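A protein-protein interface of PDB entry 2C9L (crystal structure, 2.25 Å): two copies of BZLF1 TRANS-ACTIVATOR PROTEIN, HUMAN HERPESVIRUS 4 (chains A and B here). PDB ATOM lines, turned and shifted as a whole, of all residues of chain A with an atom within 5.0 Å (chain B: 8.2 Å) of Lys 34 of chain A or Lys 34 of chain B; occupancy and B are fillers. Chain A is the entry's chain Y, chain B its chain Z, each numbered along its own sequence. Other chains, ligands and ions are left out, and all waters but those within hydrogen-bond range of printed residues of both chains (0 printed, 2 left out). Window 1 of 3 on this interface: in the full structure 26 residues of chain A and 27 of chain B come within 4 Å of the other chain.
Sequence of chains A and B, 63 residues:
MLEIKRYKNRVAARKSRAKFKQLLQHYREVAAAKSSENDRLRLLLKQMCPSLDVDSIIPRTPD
The backbone carbonyl oxygen of Lys 34 of chain A sits at hydrogen-bond distance from the side-chain amide nitrogen of Asn 38 of chain B (3.2 Å). The side-chain amino group (NZ) of Lys 34 of chain A lies within hydrogen-bond range of the backbone carbonyl oxygen (O) of Thr 61 of chain B, at 2.6 Å. NZ of Lys 34 of chain A lies within salt-bridge range of OD1 of Asp 63 of chain B (3.3 Å). NZ of Lys 34 of chain B sits at hydrogen-bond distance from OG of Ser 35 of chain A (3.4 Å). OE2 of Glu 37 of chain A lies within hydrogen-bond range of ND2 of Asn 38 of chain B, 2.6 Å away. OE2 of Glu 37 of chain A lies within salt-bridge range of NH2 of Arg 42 of chain B (3.5 Å). The side-chain hydroxyl of Thr 61 of chain B sits at hydrogen-bond distance from the side-chain carboxylate of Glu 37 of chain A. The side-chain carboxylate (OE2) of Glu 37 of chain B is in hydrogen-bond range of the side-chain amide nitrogen (ND2) of Asn 38 of chain A (2.6 Å). OD1 of Asn 38 of chain B lies close to ND2 of Asn 38 of chain A (3.0 Å). O of Thr 61 of chain A lies within hydrogen-bond range of NZ of Lys 34 of chain B (3.5 Å). The side-chain hydroxyl (OG1) of Thr 61 of chain A lies within hydrogen-bond range of the side-chain carboxylate (OE1) of Glu 37 of chain B (3.0 Å). NZ of Lys 34 of chain B lies within salt-bridge range of OD2 of Asp 63 of chain A, 2.5 Å away. OE1 of Glu 37 of chain A lies close to O of Pro 59 of chain B, at 3.4 Å.
Among the printed residues, pairs that only touch across the chains: Val 30 of chain A with Asp 63 of chain B, Lys 34 of chain A with Ser 35 of chain B, Pro 62 of chain A with Lys 34 of chain B, Asn 38 of chain A with Leu 41 of chain B, Lys 34 of chain A with Lys 34 of chain B, Val 30 of chain A with Ala 31 of chain B, Glu 37 of chain A with Arg 60 of chain B and Ala 31 of chain A with Val 30 of chain B.
The side-chain hydroxyl of Ser 35 of chain A sits at hydrogen-bond distance from the side-chain carboxylate of Asp 63 of chain A (2.8 Å). The backbone carbonyl oxygen of Ala 31 of chain B sits at hydrogen-bond distance from the side-chain hydroxyl of Ser 35 of chain B, at 3.0 Å. O of Lys 34 of chain B lies close to OD1 of Asn 38 of chain B (3.3 Å). The guanidinium group (NH1) of Arg 60 of chain B lies within salt-bridge range of the side-chain carboxylate (OD2) of Asp 39 of chain B, 3.8 Å away. The guanidinium group of Arg 42 of chain B lies within hydrogen-bond range of the backbone carbonyl oxygen of Pro 59 of chain B (3.1 Å).
Lys 34 of chain B touches its own counterpart, Lys 34 of chain A. Lys 34 of chain A touches Asp 63 of chain B, and with the chains exchanged Asp 63 of chain A touches Lys 34 of chain B. Glu 37 of chain A touches Asn 38 of chain B, and with the chains exchanged Asn 38 of chain A touches Glu 37 of chain B. Glu 37 of chain A touches Thr 61 of chain B, and with the chains exchanged Thr 61 of chain A touches Glu 37 of chain B. Of the 21 pairs that touch across the chains among the printed residues, 14 have their exchanged pair printed and touching as well.
Of the printed residues of chain B, Val 30 of chain A touches Ala 31 (3.9 Å) and Asp 63 (3.1 Å). Of chain B, only Lys 34 (3.7 Å), Ser 35 (3.1 Å), Asn 38 (3.2 Å), Thr 61 (2.6 Å) and Asp 63 (3.3 Å) come within 4 Å of Lys 34 of chain A. Printed residues of chain B within 4 Å of Ser 35 of chain A: Lys 34. Printed residues of chain B within 4 Å of Thr 61 of chain A: Lys 34 and Glu 37. Of chain A, only Lys 34, Ser 35, Thr 61, Pro 62 and Asp 63 come within 4 Å of Lys 34 of chain B. Of the printed residues of chain A, Ser 35 of chain B touches Lys 34. Pro 62 of chain B touches none of the printed residues of chain A. The nearest residue of chain B that does not touch Lys 34 of chain A is Ala 31 of chain B (4.3 Å). The nearest printed residue of chain A that does not touch Lys 34 of chain B is Asn 38 of chain A (4.5 Å). The nearest printed residue of chain B that does not touch Asn 38 of chain A is Lys 34 of chain B (4.5 Å).
Of the 21 printed residues of chain B, 12 touch a printed residue of chain A. Hydrophobic or aromatic side chains of chain B that line the printed part of chain A: Val 30, Ala 31 and Leu 41. Along chain A the printed residues that touch a printed residue of chain B span positions 30 to 63.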
ATOM      1  N   GLU A  29      -1.695 -24.420  10.780  1.00  0.00           N
ATOM      2  CA  GLU A  29      -1.131 -25.180   9.659  1.00  0.00           C
ATOM      3  C   GLU A  29      -1.322 -24.475   8.320  1.00  0.00           C
ATOM      4  O   GLU A  29      -0.418 -24.455   7.494  1.00  0.00           O
ATOM      5  CB  GLU A  29      -1.782 -26.565   9.562  1.00  0.00           C
ATOM      6  CG  GLU A  29      -1.623 -27.437  10.786  1.00  0.00           C
ATOM      7  CD  GLU A  29      -2.251 -28.808  10.599  1.00  0.00           C
ATOM      8  OE1 GLU A  29      -3.423 -28.872  10.165  1.00  0.00           O
ATOM      9  OE2 GLU A  29      -1.578 -29.819  10.894  1.00  0.00           O
ATOM     10  N   VAL A  30      -2.517 -23.934   8.106  1.00  0.00           N
ATOM     11  CA  VAL A  30      -2.843 -23.217   6.882  1.00  0.00           C
ATOM     12  C   VAL A  30      -1.989 -21.951   6.756  1.00  0.00           C
ATOM     13  O   VAL A  30      -1.519 -21.622   5.672  1.00  0.00           O
ATOM     14  CB  VAL A  30      -4.340 -22.838   6.855  1.00  0.00           C
ATOM     15  CG1 VAL A  30      -4.604 -21.765   5.814  1.00  0.00           C
ATOM     16  CG2 VAL A  30      -5.169 -24.079   6.554  1.00  0.00           C
ATOM     17  N   ALA A  31      -1.798 -21.245   7.868  1.00  0.00           N
ATOM     18  CA  ALA A  31      -0.979 -20.036   7.863  1.00  0.00           C
ATOM     19  C   ALA A  31       0.421 -20.376   7.373  1.00  0.00           C
ATOM     20  O   ALA A  31       1.012 -19.635   6.585  1.00  0.00           O
ATOM     21  CB  ALA A  31      -0.891 -19.447   9.253  1.00  0.00           C
ATOM     22  N   ALA A  32       0.944 -21.495   7.861  1.00  0.00           N
ATOM     23  CA  ALA A  32       2.277 -21.946   7.495  1.00  0.00           C
ATOM     24  C   ALA A  32       2.291 -22.400   6.035  1.00  0.00           C
ATOM     25  O   ALA A  32       3.168 -22.005   5.278  1.00  0.00           O
ATOM     26  CB  ALA A  32       2.723 -23.087   8.421  1.00  0.00           C
ATOM     27  N   ALA A  33       1.308 -23.211   5.644  1.00  0.00           N
ATOM     28  CA  ALA A  33       1.218 -23.699   4.266  1.00  0.00           C
ATOM     29  C   ALA A  33       1.120 -22.557   3.258  1.00  0.00           C
ATOM     30  O   ALA A  33       1.788 -22.585   2.232  1.00  0.00           O
ATOM     31  CB  ALA A  33       0.016 -24.634   4.107  1.00  0.00           C
ATOM     32  N   LYS A  34       0.281 -21.565   3.546  1.00  0.00           N
ATOM     33  CA  LYS A  34       0.108 -20.414   2.657  1.00  0.00           C
ATOM     34  C   LYS A  34       1.386 -19.588   2.608  1.00  0.00           C
ATOM     35  O   LYS A  34       1.736 -19.020   1.571  1.00  0.00           O
ATOM     36  CB  LYS A  34      -1.030 -19.512   3.150  1.00  0.00           C
ATOM     37  CG  LYS A  34      -2.418 -20.126   3.088  1.00  0.00           C
ATOM     38  CD  LYS A  34      -2.880 -20.346   1.658  1.00  0.00           C
ATOM     39  CE  LYS A  34      -4.355 -20.736   1.622  1.00  0.00           C
ATOM     40  NZ  LYS A  34      -4.881 -20.864   0.235  1.00  0.00           N
ATOM     41  N   SER A  35       2.079 -19.517   3.739  1.00  0.00           N
ATOM     42  CA  SER A  35       3.313 -18.754   3.815  1.00  0.00           C
ATOM     43  C   SER A  35       4.411 -19.425   2.990  1.00  0.00           C
ATOM     44  O   SER A  35       5.167 -18.751   2.298  1.00  0.00           O
ATOM     45  CB  SER A  35       3.758 -18.621   5.271  1.00  0.00           C
ATOM     46  OG  SER A  35       4.832 -17.710   5.385  1.00  0.00           O
ATOM     47  N   SER A  36       4.503 -20.749   3.063  1.00  0.00           N
ATOM     48  CA  SER A  36       5.517 -21.460   2.298  1.00  0.00           C
ATOM     49  C   SER A  36       5.176 -21.350   0.811  1.00  0.00           C
ATOM     50  O   SER A  36       6.059 -21.146  -0.017  1.00  0.00           O
ATOM     51  CB  SER A  36       5.584 -22.926   2.728  1.00  0.00           C
ATOM     52  OG  SER A  36       4.340 -23.562   2.528  1.00  0.00           O
ATOM     53  N   GLU A  37       3.896 -21.477   0.473  1.00  0.00           N
ATOM     54  CA  GLU A  37       3.478 -21.349  -0.922  1.00  0.00           C
ATOM     55  C   GLU A  37       3.844 -19.955  -1.434  1.00  0.00           C
ATOM     56  O   GLU A  37       4.298 -19.807  -2.561  1.00  0.00           O
ATOM     57  CB  GLU A  37       1.968 -21.549  -1.068  1.00  0.00           C
ATOM     58  CG  GLU A  37       1.441 -21.213  -2.465  1.00  0.00           C
ATOM     59  CD  GLU A  37      -0.075 -21.304  -2.573  1.00  0.00           C
ATOM     60  OE1 GLU A  37      -0.625 -22.401  -2.338  1.00  0.00           O
ATOM     61  OE2 GLU A  37      -0.718 -20.278  -2.896  1.00  0.00           O
ATOM     62  N   ASN A  38       3.632 -18.939  -0.600  1.00  0.00           N
ATOM     63  CA  ASN A  38       3.953 -17.558  -0.958  1.00  0.00           C
ATOM     64  C   ASN A  38       5.433 -17.480  -1.331  1.00  0.00           C
ATOM     65  O   ASN A  38       5.802 -16.816  -2.295  1.00  0.00           O
ATOM     66  CB  ASN A  38       3.645 -16.620   0.223  1.00  0.00           C
ATOM     67  CG  ASN A  38       4.013 -15.159  -0.054  1.00  0.00           C
ATOM     68  OD1 ASN A  38       5.183 -14.780  -0.013  1.00  0.00           O
ATOM     69  ND2 ASN A  38       3.005 -14.335  -0.334  1.00  0.00           N
ATOM     70  N   THR A  61       4.595  -9.744   3.784  1.00  0.00           N
ATOM     71  CA  THR A  61       3.850  -9.482   5.008  1.00  0.00           C
ATOM     72  C   THR A  61       4.517 -10.261   6.132  1.00  0.00           C
ATOM     73  O   THR A  61       5.080 -11.331   5.902  1.00  0.00           O
ATOM     74  CB  THR A  61       2.376  -9.948   4.877  1.00  0.00           C
ATOM     75  OG1 THR A  61       1.669  -9.054   4.010  1.00  0.00           O
ATOM     76  CG2 THR A  61       1.686  -9.977   6.235  1.00  0.00           C
ATOM     77  N   PRO A  62       4.485  -9.728   7.361  1.00  0.00           N
ATOM     78  CA  PRO A  62       5.114 -10.462   8.460  1.00  0.00           C
ATOM     79  C   PRO A  62       4.347 -11.749   8.743  1.00  0.00           C
ATOM     80  O   PRO A  62       3.360 -12.055   8.070  1.00  0.00           O
ATOM     81  CB  PRO A  62       5.044  -9.469   9.618  1.00  0.00           C
ATOM     82  CG  PRO A  62       3.796  -8.691   9.315  1.00  0.00           C
ATOM     83  CD  PRO A  62       3.933  -8.446   7.832  1.00  0.00           C
ATOM     84  N   ASP A  63       4.807 -12.505   9.733  1.00  0.00           N
ATOM     85  CA  ASP A  63       4.155 -13.754  10.097  1.00  0.00           C
ATOM     86  C   ASP A  63       4.119 -13.905  11.615  1.00  0.00           C
ATOM     87  O   ASP A  63       4.752 -13.078  12.306  1.00  0.00           O
ATOM     88  CB  ASP A  63       4.900 -14.939   9.478  1.00  0.00           C
ATOM     89  CG  ASP A  63       4.932 -14.886   7.960  1.00  0.00           C
ATOM     90  OD1 ASP A  63       5.526 -13.938   7.404  1.00  0.00           O
ATOM     91  OD2 ASP A  63       4.364 -15.798   7.322  1.00  0.00           O
ATOM     92  OXT ASP A  63       3.461 -14.853  12.095  1.00  0.00           O
ATOM     93  N   TYR B  27      -3.716 -16.309  13.856  1.00  0.00           N
ATOM     94  CA  TYR B  27      -3.438 -17.236  12.762  1.00  0.00           C
ATOM     95  C   TYR B  27      -4.413 -17.017  11.624  1.00  0.00           C
ATOM     96  O   TYR B  27      -4.037 -17.055  10.451  1.00  0.00           O
ATOM     97  CB  TYR B  27      -3.529 -18.687  13.244  1.00  0.00           C
ATOM     98  CG  TYR B  27      -2.406 -19.092  14.168  1.00  0.00           C
ATOM     99  CD1 TYR B  27      -2.653 -19.887  15.284  1.00  0.00           C
ATOM    100  CD2 TYR B  27      -1.098 -18.663  13.941  1.00  0.00           C
ATOM    101  CE1 TYR B  27      -1.630 -20.238  16.162  1.00  0.00           C
ATOM    102  CE2 TYR B  27      -0.065 -19.010  14.812  1.00  0.00           C
ATOM    103  CZ  TYR B  27      -0.342 -19.797  15.922  1.00  0.00           C
ATOM    104  OH  TYR B  27       0.660 -20.131  16.806  1.00  0.00           O
ATOM    105  N   ARG B  28      -5.668 -16.761  11.972  1.00  0.00           N
ATOM    106  CA  ARG B  28      -6.700 -16.545  10.971  1.00  0.00           C
ATOM    107  C   ARG B  28      -6.338 -15.346  10.098  1.00  0.00           C
ATOM    108  O   ARG B  28      -6.478 -15.386   8.866  1.00  0.00           O
ATOM    109  CB  ARG B  28      -8.042 -16.313  11.663  1.00  0.00           C
ATOM    110  CG  ARG B  28      -9.214 -17.036  11.029  1.00  0.00           C
ATOM    111  CD  ARG B  28     -10.477 -16.873  11.873  1.00  0.00           C
ATOM    112  NE  ARG B  28     -11.599 -17.629  11.325  1.00  0.00           N
ATOM    113  CZ  ARG B  28     -12.828 -17.624  11.830  1.00  0.00           C
ATOM    114  NH1 ARG B  28     -13.105 -16.901  12.906  1.00  0.00           N
ATOM    115  NH2 ARG B  28     -13.784 -18.341  11.254  1.00  0.00           N
ATOM    116  N   GLU B  29      -5.868 -14.282  10.743  1.00  0.00           N
ATOM    117  CA  GLU B  29      -5.478 -13.069  10.036  1.00  0.00           C
ATOM    118  C   GLU B  29      -4.251 -13.330   9.169  1.00  0.00           C
ATOM    119  O   GLU B  29      -4.205 -12.922   8.010  1.00  0.00           O
ATOM    120  CB  GLU B  29      -5.237 -11.933  11.045  1.00  0.00           C
ATOM    121  CG  GLU B  29      -6.551 -11.427  11.670  1.00  0.00           C
ATOM    122  CD  GLU B  29      -6.371 -10.519  12.889  1.00  0.00           C
ATOM    123  OE1 GLU B  29      -7.377  -9.924  13.332  1.00  0.00           O
ATOM    124  OE2 GLU B  29      -5.243 -10.404  13.413  1.00  0.00           O
ATOM    125  N   VAL B  30      -3.260 -14.024   9.717  1.00  0.00           N
ATOM    126  CA  VAL B  30      -2.065 -14.342   8.937  1.00  0.00           C
ATOM    127  C   VAL B  30      -2.457 -15.161   7.705  1.00  0.00           C
ATOM    128  O   VAL B  30      -2.026 -14.873   6.591  1.00  0.00           O
ATOM    129  CB  VAL B  30      -1.056 -15.153   9.766  1.00  0.00           C
ATOM    130  CG1 VAL B  30       0.086 -15.621   8.888  1.00  0.00           C
ATOM    131  CG2 VAL B  30      -0.534 -14.304  10.914  1.00  0.00           C
ATOM    132  N   ALA B  31      -3.291 -16.175   7.913  1.00  0.00           N
ATOM    133  CA  ALA B  31      -3.730 -17.046   6.829  1.00  0.00           C
ATOM    134  C   ALA B  31      -4.454 -16.271   5.738  1.00  0.00           C
ATOM    135  O   ALA B  31      -4.239 -16.511   4.548  1.00  0.00           O
ATOM    136  CB  ALA B  31      -4.642 -18.163   7.384  1.00  0.00           C
ATOM    137  N   ALA B  32      -5.314 -15.346   6.147  1.00  0.00           N
ATOM    138  CA  ALA B  32      -6.072 -14.528   5.206  1.00  0.00           C
ATOM    139  C   ALA B  32      -5.142 -13.564   4.481  1.00  0.00           C
ATOM    140  O   ALA B  32      -5.272 -13.351   3.276  1.00  0.00           O
ATOM    141  CB  ALA B  32      -7.156 -13.749   5.944  1.00  0.00           C
ATOM    142  N   ALA B  33      -4.210 -12.975   5.222  1.00  0.00           N
ATOM    143  CA  ALA B  33      -3.258 -12.040   4.636  1.00  0.00           C
ATOM    144  C   ALA B  33      -2.431 -12.750   3.561  1.00  0.00           C
ATOM    145  O   ALA B  33      -2.309 -12.259   2.440  1.00  0.00           O
ATOM    146  CB  ALA B  33      -2.340 -11.466   5.722  1.00  0.00           C
ATOM    147  N   LYS B  34      -1.870 -13.908   3.903  1.00  0.00           N
ATOM    148  CA  LYS B  34      -1.057 -14.668   2.951  1.00  0.00           C
ATOM    149  C   LYS B  34      -1.837 -15.099   1.714  1.00  0.00           C
ATOM    150  O   LYS B  34      -1.331 -15.007   0.594  1.00  0.00           O
ATOM    151  CB  LYS B  34      -0.452 -15.899   3.631  1.00  0.00           C
ATOM    152  CG  LYS B  34       0.469 -15.550   4.779  1.00  0.00           C
ATOM    153  CD  LYS B  34       1.532 -14.558   4.330  1.00  0.00           C
ATOM    154  CE  LYS B  34       2.437 -14.154   5.484  1.00  0.00           C
ATOM    155  NZ  LYS B  34       3.868 -14.502   5.202  1.00  0.00           N
ATOM    156  N   SER B  35      -3.067 -15.566   1.919  1.00  0.00           N
ATOM    157  CA  SER B  35      -3.914 -16.007   0.813  1.00  0.00           C
ATOM    158  C   SER B  35      -4.142 -14.919  -0.225  1.00  0.00           C
ATOM    159  O   SER B  35      -4.046 -15.172  -1.424  1.00  0.00           O
ATOM    160  CB  SER B  35      -5.269 -16.493   1.333  1.00  0.00           C
ATOM    161  OG  SER B  35      -5.144 -17.730   2.009  1.00  0.00           O
ATOM    162  N   SER B  36      -4.459 -13.714   0.231  1.00  0.00           N
ATOM    163  CA  SER B  36      -4.702 -12.605  -0.682  1.00  0.00           C
ATOM    164  C   SER B  36      -3.419 -12.253  -1.428  1.00  0.00           C
ATOM    165  O   SER B  36      -3.443 -11.921  -2.612  1.00  0.00           O
ATOM    166  CB  SER B  36      -5.206 -11.384   0.089  1.00  0.00           C
ATOM    167  OG  SER B  36      -4.261 -10.966   1.054  1.00  0.00           O
ATOM    168  N   GLU B  37      -2.298 -12.333  -0.723  1.00  0.00           N
ATOM    169  CA  GLU B  37      -1.004 -12.037  -1.318  1.00  0.00           C
ATOM    170  C   GLU B  37      -0.698 -13.073  -2.393  1.00  0.00           C
ATOM    171  O   GLU B  37      -0.233 -12.737  -3.482  1.00  0.00           O
ATOM    172  CB  GLU B  37       0.077 -12.067  -0.236  1.00  0.00           C
ATOM    173  CG  GLU B  37       1.421 -11.498  -0.650  1.00  0.00           C
ATOM    174  CD  GLU B  37       2.368 -11.367   0.530  1.00  0.00           C
ATOM    175  OE1 GLU B  37       1.990 -10.711   1.524  1.00  0.00           O
ATOM    176  OE2 GLU B  37       3.486 -11.919   0.466  1.00  0.00           O
ATOM    177  N   ASN B  38      -0.972 -14.335  -2.083  1.00  0.00           N
ATOM    178  CA  ASN B  38      -0.722 -15.427  -3.017  1.00  0.00           C
ATOM    179  C   ASN B  38      -1.571 -15.325  -4.273  1.00  0.00           C
ATOM    180  O   ASN B  38      -1.133 -15.705  -5.355  1.00  0.00           O
ATOM    181  CB  ASN B  38      -0.968 -16.770  -2.333  1.00  0.00           C
ATOM    182  CG  ASN B  38       0.221 -17.227  -1.511  1.00  0.00           C
ATOM    183  OD1 ASN B  38       1.083 -16.425  -1.137  1.00  0.00           O
ATOM    184  ND2 ASN B  38       0.272 -18.521  -1.218  1.00  0.00           N
ATOM    185  N   ASP B  39      -2.789 -14.816  -4.134  1.00  0.00           N
ATOM    186  CA  ASP B  39      -3.660 -14.675  -5.288  1.00  0.00           C
ATOM    187  C   ASP B  39      -3.118 -13.580  -6.192  1.00  0.00           C
ATOM    188  O   ASP B  39      -3.226 -13.670  -7.411  1.00  0.00           O
ATOM    189  CB  ASP B  39      -5.080 -14.348  -4.841  1.00  0.00           C
ATOM    190  CG  ASP B  39      -5.707 -15.471  -4.046  1.00  0.00           C
ATOM    191  OD1 ASP B  39      -6.846 -15.302  -3.570  1.00  0.00           O
ATOM    192  OD2 ASP B  39      -5.055 -16.528  -3.901  1.00  0.00           O
ATOM    193  N   ARG B  40      -2.527 -12.552  -5.591  1.00  0.00           N
ATOM    194  CA  ARG B  40      -1.954 -11.456  -6.364  1.00  0.00           C
ATOM    195  C   ARG B  40      -0.695 -11.936  -7.088  1.00  0.00           C
ATOM    196  O   ARG B  40      -0.404 -11.499  -8.201  1.00  0.00           O
ATOM    197  CB  ARG B  40      -1.612 -10.268  -5.458  1.00  0.00           C
ATOM    198  CG  ARG B  40      -2.814  -9.649  -4.756  1.00  0.00           C
ATOM    199  CD  ARG B  40      -2.578  -8.177  -4.426  1.00  0.00           C
ATOM    200  NE  ARG B  40      -1.517  -7.961  -3.442  1.00  0.00           N
ATOM    201  CZ  ARG B  40      -1.639  -8.198  -2.138  1.00  0.00           C
ATOM    202  NH1 ARG B  40      -2.778  -8.663  -1.645  1.00  0.00           N
ATOM    203  NH2 ARG B  40      -0.621  -7.959  -1.322  1.00  0.00           N
ATOM    204  N   LEU B  41       0.046 -12.838  -6.450  1.00  0.00           N
ATOM    205  CA  LEU B  41       1.260 -13.381  -7.048  1.00  0.00           C
ATOM    206  C   LEU B  41       0.899 -14.279  -8.221  1.00  0.00           C
ATOM    207  O   LEU B  41       1.544 -14.227  -9.264  1.00  0.00           O
ATOM    208  CB  LEU B  41       2.060 -14.181  -6.015  1.00  0.00           C
ATOM    209  CG  LEU B  41       2.791 -13.370  -4.945  1.00  0.00           C
ATOM    210  CD1 LEU B  41       3.208 -14.280  -3.801  1.00  0.00           C
ATOM    211  CD2 LEU B  41       3.997 -12.680  -5.567  1.00  0.00           C
ATOM    212  N   ARG B  42      -0.134 -15.100  -8.044  1.00  0.00           N
ATOM    213  CA  ARG B  42      -0.587 -16.005  -9.098  1.00  0.00           C
ATOM    214  C   ARG B  42      -1.088 -15.247 -10.318  1.00  0.00           C
ATOM    215  O   ARG B  42      -0.938 -15.707 -11.450  1.00  0.00           O
ATOM    216  CB  ARG B  42      -1.707 -16.907  -8.586  1.00  0.00           C
ATOM    217  CG  ARG B  42      -1.231 -18.034  -7.708  1.00  0.00           C
ATOM    218  CD  ARG B  42      -2.401 -18.782  -7.100  1.00  0.00           C
ATOM    219  NE  ARG B  42      -1.939 -19.894  -6.280  1.00  0.00           N
ATOM    220  CZ  ARG B  42      -1.412 -21.012  -6.767  1.00  0.00           C
ATOM    221  NH1 ARG B  42      -1.289 -21.173  -8.079  1.00  0.00           N
ATOM    222  NH2 ARG B  42      -0.994 -21.958  -5.940  1.00  0.00           N
ATOM    223  N   PRO B  59      -0.016 -25.989  -6.901  1.00  0.00           N
ATOM    224  CA  PRO B  59      -1.475 -25.938  -6.773  1.00  0.00           C
ATOM    225  C   PRO B  59      -1.924 -25.037  -5.629  1.00  0.00           C
ATOM    226  O   PRO B  59      -1.183 -24.825  -4.670  1.00  0.00           O
ATOM    227  CB  PRO B  59      -1.851 -27.400  -6.553  1.00  0.00           C
ATOM    228  CG  PRO B  59      -0.657 -27.943  -5.834  1.00  0.00           C
ATOM    229  CD  PRO B  59       0.486 -27.343  -6.614  1.00  0.00           C
ATOM    230  N   ARG B  60      -3.136 -24.504  -5.741  1.00  0.00           N
ATOM    231  CA  ARG B  60      -3.688 -23.618  -4.721  1.00  0.00           C
ATOM    232  C   ARG B  60      -3.883 -24.338  -3.391  1.00  0.00           C
ATOM    233  O   ARG B  60      -4.423 -25.443  -3.350  1.00  0.00           O
ATOM    234  CB  ARG B  60      -5.034 -23.059  -5.189  1.00  0.00           C
ATOM    235  CG  ARG B  60      -4.954 -22.152  -6.405  1.00  0.00           C
ATOM    236  CD  ARG B  60      -6.345 -21.832  -6.939  1.00  0.00           C
ATOM    237  NE  ARG B  60      -6.309 -20.851  -8.020  1.00  0.00           N
ATOM    238  CZ  ARG B  60      -6.050 -19.557  -7.848  1.00  0.00           C
ATOM    239  NH1 ARG B  60      -5.807 -19.081  -6.634  1.00  0.00           N
ATOM    240  NH2 ARG B  60      -6.030 -18.740  -8.893  1.00  0.00           N
ATOM    241  N   THR B  61      -3.465 -23.715  -2.296  1.00  0.00           N
ATOM    242  CA  THR B  61      -3.628 -24.306  -0.961  1.00  0.00           C
ATOM    243  C   THR B  61      -5.109 -24.231  -0.545  1.00  0.00           C
ATOM    244  O   THR B  61      -5.710 -23.164  -0.570  1.00  0.00           O
ATOM    245  CB  THR B  61      -2.775 -23.543   0.083  1.00  0.00           C
ATOM    246  OG1 THR B  61      -1.386 -23.611  -0.276  1.00  0.00           O
ATOM    247  CG2 THR B  61      -2.963 -24.137   1.462  1.00  0.00           C
ATOM    248  N   PRO B  62      -5.715 -25.399  -0.197  1.00  0.00           N
ATOM    249  CA  PRO B  62      -7.110 -25.562   0.229  1.00  0.00           C
ATOM    250  C   PRO B  62      -7.390 -24.810   1.522  1.00  0.00           C
ATOM    251  O   PRO B  62      -7.475 -25.403   2.604  1.00  0.00           O
ATOM    252  CB  PRO B  62      -7.252 -27.091   0.368  1.00  0.00           C
ATOM    253  CG  PRO B  62      -6.272 -27.596  -0.614  1.00  0.00           C
ATOM    254  CD  PRO B  62      -5.082 -26.701  -0.376  1.00  0.00           C
ATOM    255  N   ASP B  63      -7.445 -23.489   1.359  1.00  0.00           N
ATOM    256  CA  ASP B  63      -7.771 -22.443   2.339  1.00  0.00           C
ATOM    257  C   ASP B  63      -8.077 -23.038   3.701  1.00  0.00           C
ATOM    258  O   ASP B  63      -9.254 -22.804   4.055  1.00  0.00           O
ATOM    259  CB  ASP B  63      -9.077 -21.750   1.893  1.00  0.00           C
ATOM    260  CG  ASP B  63      -9.084 -21.455   0.454  1.00  0.00           C
ATOM    261  OD1 ASP B  63      -8.134 -20.765   0.077  1.00  0.00           O
ATOM    262  OD2 ASP B  63     -10.003 -21.891  -0.276  1.00  0.00           O
ATOM    263  OXT ASP B  63      -7.270 -23.716   4.362  1.00  0.00           O
